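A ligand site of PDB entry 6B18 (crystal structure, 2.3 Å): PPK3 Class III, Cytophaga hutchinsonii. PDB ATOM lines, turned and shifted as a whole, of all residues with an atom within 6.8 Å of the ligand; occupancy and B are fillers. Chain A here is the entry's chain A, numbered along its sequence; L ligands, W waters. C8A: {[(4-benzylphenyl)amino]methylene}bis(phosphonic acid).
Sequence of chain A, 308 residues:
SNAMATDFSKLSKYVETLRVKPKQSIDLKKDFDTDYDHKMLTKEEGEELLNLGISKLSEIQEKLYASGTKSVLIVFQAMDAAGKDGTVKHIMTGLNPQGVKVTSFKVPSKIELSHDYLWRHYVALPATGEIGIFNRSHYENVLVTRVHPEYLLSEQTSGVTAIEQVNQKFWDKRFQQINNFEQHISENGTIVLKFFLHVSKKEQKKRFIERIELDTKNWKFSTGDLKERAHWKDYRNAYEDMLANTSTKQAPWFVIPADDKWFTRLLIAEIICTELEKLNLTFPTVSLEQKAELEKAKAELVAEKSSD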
ATOM      1  N   ASP A  80      25.231 -15.097   5.442  1.00  0.00           N
ATOM      2  CA  ASP A  80      24.498 -14.683   6.660  1.00  0.00           C
ATOM      3  C   ASP A  80      24.491 -13.179   6.766  1.00  0.00           C
ATOM      4  O   ASP A  80      25.428 -12.538   6.343  1.00  0.00           O
ATOM      5  CB  ASP A  80      25.120 -15.249   7.932  1.00  0.00           C
ATOM      6  CG  ASP A  80      25.082 -16.757   7.966  1.00  0.00           C
ATOM      7  OD1 ASP A  80      24.000 -17.354   7.754  1.00  0.00           O
ATOM      8  OD2 ASP A  80      26.146 -17.370   8.198  1.00  0.00           O
ATOM      9  N   ALA A  81      23.398 -12.654   7.287  1.00  0.00           N
ATOM     10  CA  ALA A  81      23.160 -11.233   7.476  1.00  0.00           C
ATOM     11  C   ALA A  81      22.992 -10.425   6.209  1.00  0.00           C
ATOM     12  O   ALA A  81      23.053  -9.217   6.269  1.00  0.00           O
ATOM     13  CB  ALA A  81      24.240 -10.613   8.357  1.00  0.00           C
ATOM     14  N   GLY A  83      20.155 -10.189   4.766  1.00  0.00           N
ATOM     15  CA  GLY A  83      18.745  -9.714   4.847  1.00  0.00           C
ATOM     16  C   GLY A  83      17.715 -10.704   4.314  1.00  0.00           C
ATOM     17  O   GLY A  83      16.556 -10.346   4.115  1.00  0.00           O
ATOM     18  N   LYS A  84      18.136 -11.955   4.129  1.00  0.00           N
ATOM     19  CA  LYS A  84      17.328 -12.980   3.462  1.00  0.00           C
ATOM     20  C   LYS A  84      16.011 -13.306   4.200  1.00  0.00           C
ATOM     21  O   LYS A  84      14.920 -13.205   3.610  1.00  0.00           O
ATOM     22  CB  LYS A  84      18.191 -14.213   3.280  1.00  0.00           C
ATOM     23  CG  LYS A  84      17.501 -15.375   2.609  1.00  0.00           C
ATOM     24  CD  LYS A  84      18.490 -16.418   2.079  1.00  0.00           C
ATOM     25  CE  LYS A  84      19.400 -16.999   3.154  1.00  0.00           C
ATOM     26  NZ  LYS A  84      18.620 -17.430   4.339  1.00  0.00           N
ATOM     27  N   ASP A  85      16.115 -13.645   5.494  1.00  0.00           N
ATOM     28  CA  ASP A  85      14.935 -13.888   6.344  1.00  0.00           C
ATOM     29  C   ASP A  85      13.979 -12.692   6.433  1.00  0.00           C
ATOM     30  O   ASP A  85      12.771 -12.858   6.346  1.00  0.00           O
ATOM     31  CB  ASP A  85      15.344 -14.312   7.764  1.00  0.00           C
ATOM     32  CG  ASP A  85      15.989 -15.713   7.830  1.00  0.00           C
ATOM     33  OD1 ASP A  85      16.172 -16.412   6.809  1.00  0.00           O
ATOM     34  OD2 ASP A  85      16.355 -16.114   8.952  1.00  0.00           O
ATOM     35  N   GLY A  86      14.532 -11.490   6.585  1.00  0.00           N
ATOM     36  CA  GLY A  86      13.720 -10.272   6.602  1.00  0.00           C
ATOM     37  C   GLY A  86      12.981 -10.024   5.311  1.00  0.00           C
ATOM     38  O   GLY A  86      11.802  -9.717   5.329  1.00  0.00           O
ATOM     39  N   ARG A 207      26.686  -5.484  10.342  1.00  0.00           N
ATOM     40  CA  ARG A 207      25.436  -6.069  10.799  1.00  0.00           C
ATOM     41  C   ARG A 207      25.632  -7.054  11.927  1.00  0.00           C
ATOM     42  O   ARG A 207      24.903  -6.996  12.910  1.00  0.00           O
ATOM     43  CB  ARG A 207      24.722  -6.722   9.623  1.00  0.00           C
ATOM     44  CG  ARG A 207      24.202  -5.707   8.637  1.00  0.00           C
ATOM     45  CD  ARG A 207      23.568  -6.386   7.450  1.00  0.00           C
ATOM     46  NE  ARG A 207      23.137  -5.386   6.494  1.00  0.00           N
ATOM     47  CZ  ARG A 207      22.618  -5.623   5.302  1.00  0.00           C
ATOM     48  NH1 ARG A 207      22.431  -6.859   4.856  1.00  0.00           N
ATOM     49  NH2 ARG A 207      22.262  -4.590   4.538  1.00  0.00           N
ATOM     50  N   PHE A 208      26.616  -7.927  11.790  1.00  0.00           N
ATOM     51  CA  PHE A 208      27.044  -8.820  12.890  1.00  0.00           C
ATOM     52  C   PHE A 208      27.305  -8.057  14.196  1.00  0.00           C
ATOM     53  O   PHE A 208      26.779  -8.398  15.246  1.00  0.00           O
ATOM     54  CB  PHE A 208      28.322  -9.581  12.503  1.00  0.00           C
ATOM     55  CG  PHE A 208      28.133 -10.823  11.661  1.00  0.00           C
ATOM     56  CD1 PHE A 208      26.903 -11.229  11.153  1.00  0.00           C
ATOM     57  CD2 PHE A 208      29.252 -11.583  11.315  1.00  0.00           C
ATOM     58  CE1 PHE A 208      26.799 -12.397  10.379  1.00  0.00           C
ATOM     59  CE2 PHE A 208      29.149 -12.729  10.537  1.00  0.00           C
ATOM     60  CZ  PHE A 208      27.916 -13.133  10.069  1.00  0.00           C
ATOM     61  N   ILE A 209      28.116  -7.006  14.133  1.00  0.00           N
ATOM     62  CA  ILE A 209      28.406  -6.193  15.321  1.00  0.00           C
ATOM     63  C   ILE A 209      27.155  -5.560  15.893  1.00  0.00           C
ATOM     64  O   ILE A 209      26.917  -5.607  17.104  1.00  0.00           O
ATOM     65  CB  ILE A 209      29.486  -5.142  15.035  1.00  0.00           C
ATOM     66  CG1 ILE A 209      30.831  -5.849  14.906  1.00  0.00           C
ATOM     67  CG2 ILE A 209      29.547  -4.096  16.136  1.00  0.00           C
ATOM     68  CD1 ILE A 209      31.932  -4.983  14.329  1.00  0.00           C
ATOM     69  N   ARG A 211      24.074  -6.647  15.703  1.00  0.00           N
ATOM     70  CA  ARG A 211      23.329  -7.739  16.357  1.00  0.00           C
ATOM     71  C   ARG A 211      23.951  -8.106  17.705  1.00  0.00           C
ATOM     72  O   ARG A 211      23.226  -8.306  18.699  1.00  0.00           O
ATOM     73  CB  ARG A 211      23.312  -9.050  15.532  1.00  0.00           C
ATOM     74  CG  ARG A 211      22.512  -9.136  14.230  1.00  0.00           C
ATOM     75  CD  ARG A 211      22.955 -10.393  13.452  1.00  0.00           C
ATOM     76  NE  ARG A 211      22.099 -10.757  12.307  1.00  0.00           N
ATOM     77  CZ  ARG A 211      22.282 -11.827  11.509  1.00  0.00           C
ATOM     78  NH1 ARG A 211      23.291 -12.687  11.714  1.00  0.00           N
ATOM     79  NH2 ARG A 211      21.433 -12.039  10.505  1.00  0.00           N
ATOM     80  N   ILE A 212      25.270  -8.257  17.720  1.00  0.00           N
ATOM     81  CA  ILE A 212      25.995  -8.532  18.980  1.00  0.00           C
ATOM     82  C   ILE A 212      25.707  -7.499  20.046  1.00  0.00           C
ATOM     83  O   ILE A 212      25.586  -7.848  21.190  1.00  0.00           O
ATOM     84  CB  ILE A 212      27.511  -8.656  18.769  1.00  0.00           C
ATOM     85  CG1 ILE A 212      27.811  -9.997  18.104  1.00  0.00           C
ATOM     86  CG2 ILE A 212      28.281  -8.588  20.082  1.00  0.00           C
ATOM     87  CD1 ILE A 212      29.236 -10.142  17.634  1.00  0.00           C
ATOM     88  N   LYS A 217      18.326  -9.074  20.552  1.00  0.00           N
ATOM     89  CA  LYS A 217      18.726 -10.133  19.590  1.00  0.00           C
ATOM     90  C   LYS A 217      19.844 -11.106  20.054  1.00  0.00           C
ATOM     91  O   LYS A 217      20.016 -12.192  19.492  1.00  0.00           O
ATOM     92  CB  LYS A 217      19.211  -9.473  18.292  1.00  0.00           C
ATOM     93  CG  LYS A 217      18.177  -8.559  17.634  1.00  0.00           C
ATOM     94  CD  LYS A 217      18.660  -7.968  16.307  1.00  0.00           C
ATOM     95  CE  LYS A 217      17.578  -7.052  15.720  1.00  0.00           C
ATOM     96  NZ  LYS A 217      17.760  -6.690  14.284  1.00  0.00           N
ATOM     97  N   ASN A 218      20.621 -10.686  21.044  1.00  0.00           N
ATOM     98  CA  ASN A 218      21.811 -11.411  21.545  1.00  0.00           C
ATOM     99  C   ASN A 218      21.697 -12.883  21.800  1.00  0.00           C
ATOM    100  O   ASN A 218      22.639 -13.623  21.555  1.00  0.00           O
ATOM    101  CB  ASN A 218      22.249 -10.784  22.903  1.00  0.00           C
ATOM    102  CG  ASN A 218      23.137  -9.604  22.698  1.00  0.00           C
ATOM    103  OD1 ASN A 218      23.193  -8.696  23.509  1.00  0.00           O
ATOM    104  ND2 ASN A 218      23.839  -9.609  21.571  1.00  0.00           N
ATOM    105  N   TRP A 219      20.576 -13.269  22.409  1.00  0.00           N
ATOM    106  CA  TRP A 219      20.338 -14.661  22.809  1.00  0.00           C
ATOM    107  C   TRP A 219      20.305 -15.671  21.663  1.00  0.00           C
ATOM    108  O   TRP A 219      20.436 -16.868  21.928  1.00  0.00           O
ATOM    109  CB  TRP A 219      19.025 -14.755  23.596  1.00  0.00           C
ATOM    110  CG  TRP A 219      17.794 -14.322  22.814  1.00  0.00           C
ATOM    111  CD1 TRP A 219      17.232 -13.072  22.779  1.00  0.00           C
ATOM    112  CD2 TRP A 219      16.976 -15.146  21.969  1.00  0.00           C
ATOM    113  NE1 TRP A 219      16.122 -13.067  21.972  1.00  0.00           N
ATOM    114  CE2 TRP A 219      15.940 -14.332  21.465  1.00  0.00           C
ATOM    115  CE3 TRP A 219      17.021 -16.499  21.597  1.00  0.00           C
ATOM    116  CZ2 TRP A 219      14.956 -14.808  20.611  1.00  0.00           C
ATOM    117  CZ3 TRP A 219      16.047 -16.989  20.747  1.00  0.00           C
ATOM    118  CH2 TRP A 219      15.025 -16.146  20.256  1.00  0.00           C
ATOM    119  N   LYS A 220      20.121 -15.189  20.426  1.00  0.00           N
ATOM    120  CA  LYS A 220      20.087 -16.053  19.236  1.00  0.00           C
ATOM    121  C   LYS A 220      21.447 -16.504  18.758  1.00  0.00           C
ATOM    122  O   LYS A 220      21.540 -17.423  17.923  1.00  0.00           O
ATOM    123  CB  LYS A 220      19.444 -15.306  18.073  1.00  0.00           C
ATOM    124  CG  LYS A 220      18.005 -14.906  18.311  1.00  0.00           C
ATOM    125  CD  LYS A 220      17.561 -13.933  17.249  1.00  0.00           C
ATOM    126  CE  LYS A 220      16.105 -14.119  16.867  1.00  0.00           C
ATOM    127  NZ  LYS A 220      15.970 -13.910  15.394  1.00  0.00           N
ATOM    128  N   PHE A 221      22.513 -15.847  19.225  1.00  0.00           N
ATOM    129  CA  PHE A 221      23.862 -16.276  18.889  1.00  0.00           C
ATOM    130  C   PHE A 221      24.175 -17.618  19.540  1.00  0.00           C
ATOM    131  O   PHE A 221      23.975 -17.789  20.756  1.00  0.00           O
ATOM    132  CB  PHE A 221      24.907 -15.254  19.326  1.00  0.00           C
ATOM    133  CG  PHE A 221      26.326 -15.740  19.214  1.00  0.00           C
ATOM    134  CD1 PHE A 221      26.929 -16.417  20.268  1.00  0.00           C
ATOM    135  CD2 PHE A 221      27.062 -15.536  18.040  1.00  0.00           C
ATOM    136  CE1 PHE A 221      28.242 -16.865  20.169  1.00  0.00           C
ATOM    137  CE2 PHE A 221      28.379 -15.991  17.934  1.00  0.00           C
ATOM    138  CZ  PHE A 221      28.973 -16.656  19.002  1.00  0.00           C
ATOM    139  N   SER A 222      24.681 -18.552  18.736  1.00  0.00           N
ATOM    140  CA  SER A 222      25.193 -19.847  19.193  1.00  0.00           C
ATOM    141  C   SER A 222      26.652 -19.898  18.828  1.00  0.00           C
ATOM    142  O   SER A 222      27.127 -19.168  17.920  1.00  0.00           O
ATOM    143  CB  SER A 222      24.472 -21.026  18.515  1.00  0.00           C
ATOM    144  OG  SER A 222      23.180 -20.677  18.030  1.00  0.00           O
ATOM    145  N   ASP A 225      28.690 -19.167  15.138  1.00  0.00           N
ATOM    146  CA  ASP A 225      27.856 -18.512  14.124  1.00  0.00           C
ATOM    147  C   ASP A 225      28.637 -17.634  13.125  1.00  0.00           C
ATOM    148  O   ASP A 225      28.107 -17.287  12.091  1.00  0.00           O
ATOM    149  CB  ASP A 225      26.752 -17.663  14.768  1.00  0.00           C
ATOM    150  CG  ASP A 225      25.594 -18.512  15.319  1.00  0.00           C
ATOM    151  OD1 ASP A 225      25.709 -19.760  15.360  1.00  0.00           O
ATOM    152  OD2 ASP A 225      24.567 -17.891  15.737  1.00  0.00           O
ATOM    153  N   LEU A 226      29.865 -17.254  13.458  1.00  0.00           N
ATOM    154  CA  LEU A 226      30.734 -16.489  12.550  1.00  0.00           C
ATOM    155  C   LEU A 226      31.655 -17.354  11.714  1.00  0.00           C
ATOM    156  O   LEU A 226      32.397 -16.826  10.905  1.00  0.00           O
ATOM    157  CB  LEU A 226      31.641 -15.544  13.344  1.00  0.00           C
ATOM    158  CG  LEU A 226      31.088 -14.196  13.793  1.00  0.00           C
ATOM    159  CD1 LEU A 226      29.713 -14.271  14.456  1.00  0.00           C
ATOM    160  CD2 LEU A 226      32.131 -13.598  14.714  1.00  0.00           C
ATOM    161  N   LYS A 261      18.805  -2.394   2.574  1.00  0.00           N
ATOM    162  CA  LYS A 261      17.728  -3.370   2.670  1.00  0.00           C
ATOM    163  C   LYS A 261      16.424  -2.998   2.002  1.00  0.00           C
ATOM    164  O   LYS A 261      15.776  -3.859   1.373  1.00  0.00           O
ATOM    165  CB  LYS A 261      17.438  -3.716   4.122  1.00  0.00           C
ATOM    166  CG  LYS A 261      18.515  -4.578   4.731  1.00  0.00           C
ATOM    167  CD  LYS A 261      18.179  -4.884   6.160  1.00  0.00           C
ATOM    168  CE  LYS A 261      19.177  -5.852   6.751  1.00  0.00           C
ATOM    169  NZ  LYS A 261      18.909  -5.954   8.207  1.00  0.00           N
HETATM  170  C10 C8A L   1      21.217 -13.687  15.260  1.00  0.00           C
HETATM  171  C13 C8A L   1      24.246 -12.748  16.442  1.00  0.00           C
HETATM  172  C15 C8A L   1      26.067 -12.599  14.888  1.00  0.00           C
HETATM  173  C17 C8A L   1      24.272 -14.142  14.495  1.00  0.00           C
HETATM  174  O01 C8A L   1      17.844  -8.421  11.278  1.00  0.00           O
HETATM  175  P02 C8A L   1      18.582  -9.707  11.594  1.00  0.00           P
HETATM  176  O03 C8A L   1      18.491 -10.648  10.405  1.00  0.00           O
HETATM  177  O04 C8A L   1      20.026  -9.393  11.895  1.00  0.00           O
HETATM  178  C05 C8A L   1      17.805 -10.500  13.070  1.00  0.00           C
HETATM  179  N06 C8A L   1      18.068 -11.936  12.990  1.00  0.00           N
HETATM  180  C07 C8A L   1      19.181 -12.531  13.761  1.00  0.00           C
HETATM  181  C08 C8A L   1      19.729 -11.839  14.859  1.00  0.00           C
HETATM  182  C09 C8A L   1      20.745 -12.419  15.594  1.00  0.00           C
HETATM  183  C11 C8A L   1      22.337 -14.328  16.079  1.00  0.00           C
HETATM  184  C12 C8A L   1      23.660 -13.724  15.656  1.00  0.00           C
HETATM  185  C14 C8A L   1      25.452 -12.189  16.055  1.00  0.00           C
HETATM  186  C16 C8A L   1      25.478 -13.582  14.107  1.00  0.00           C
HETATM  187  C18 C8A L   1      20.666 -14.374  14.186  1.00  0.00           C
HETATM  188  C19 C8A L   1      19.643 -13.808  13.444  1.00  0.00           C
HETATM  189  P20 C8A L   1      15.966 -10.268  13.198  1.00  0.00           P
HETATM  190  O21 C8A L   1      15.391  -9.953  11.837  1.00  0.00           O
HETATM  191  O22 C8A L   1      15.671  -9.124  14.141  1.00  0.00           O
HETATM  192  O23 C8A L   1      15.328 -11.538  13.739  1.00  0.00           O
HETATM  193  O   HOH W   1      13.569  -8.436   9.556  1.00  0.00           O
HETATM  194  O   HOH W   2      13.501 -11.434   9.829  1.00  0.00           O
HETATM  195  O   HOH W   3      21.280  -7.454  10.186  1.00  0.00           O
HETATM  196  O   HOH W   4      18.480 -13.623  10.283  1.00  0.00           O
HETATM  197  O   HOH W   5      17.001 -10.657   7.714  1.00  0.00           O
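An oxygen (O22) of the ligand is in salt-bridge range of the side-chain amino group (NZ) of Lys 217, 3.2 Å away. The guanidinium group (NE) of Arg 211 is in salt-bridge range of an oxygen (O04) of the ligand (2.5 Å). O23 of the ligand lies within salt-bridge range of NZ of Lys 220, at 3.0 Å.
The backbone carbonyl oxygen (O) of Arg 211 is in hydrogen-bond range of the side-chain amide nitrogen (ND2) of Asn 218, at 3.2 Å. The side-chain carboxylate (OD2) of Asp 225 lies within hydrogen-bond range of the backbone NH (N) of Ser 222 (3.1 Å). O of Ile 212 is in hydrogen-bond range of ND2 of Asn 218 (2.5 Å).
Residues that only touch the ligand: Ile 212 (3.8 Å), Phe 221 (3.5 Å) and Asp 225 (3.96 Å). Hydrophobic or aromatic side chains within 4 Å of the ligand: Ile 212 and Phe 221.
Water W3 bridges an oxygen (O04) of the ligand and the side-chain amino group (NZ) of Lys 261. Water W4 lies within hydrogen-bond range of an oxygen (O03) of the ligand (3.0 Å) and the guanidinium group of Arg 211 (3.4 Å). Water W5 bridges N of Gly 86 (2.8 Å) and O03 of the ligand (3.1 Å). Water W2 lies within hydrogen-bond range of O21 of the ligand (3.1 Å) and N of Gly 86 (3.4 Å).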
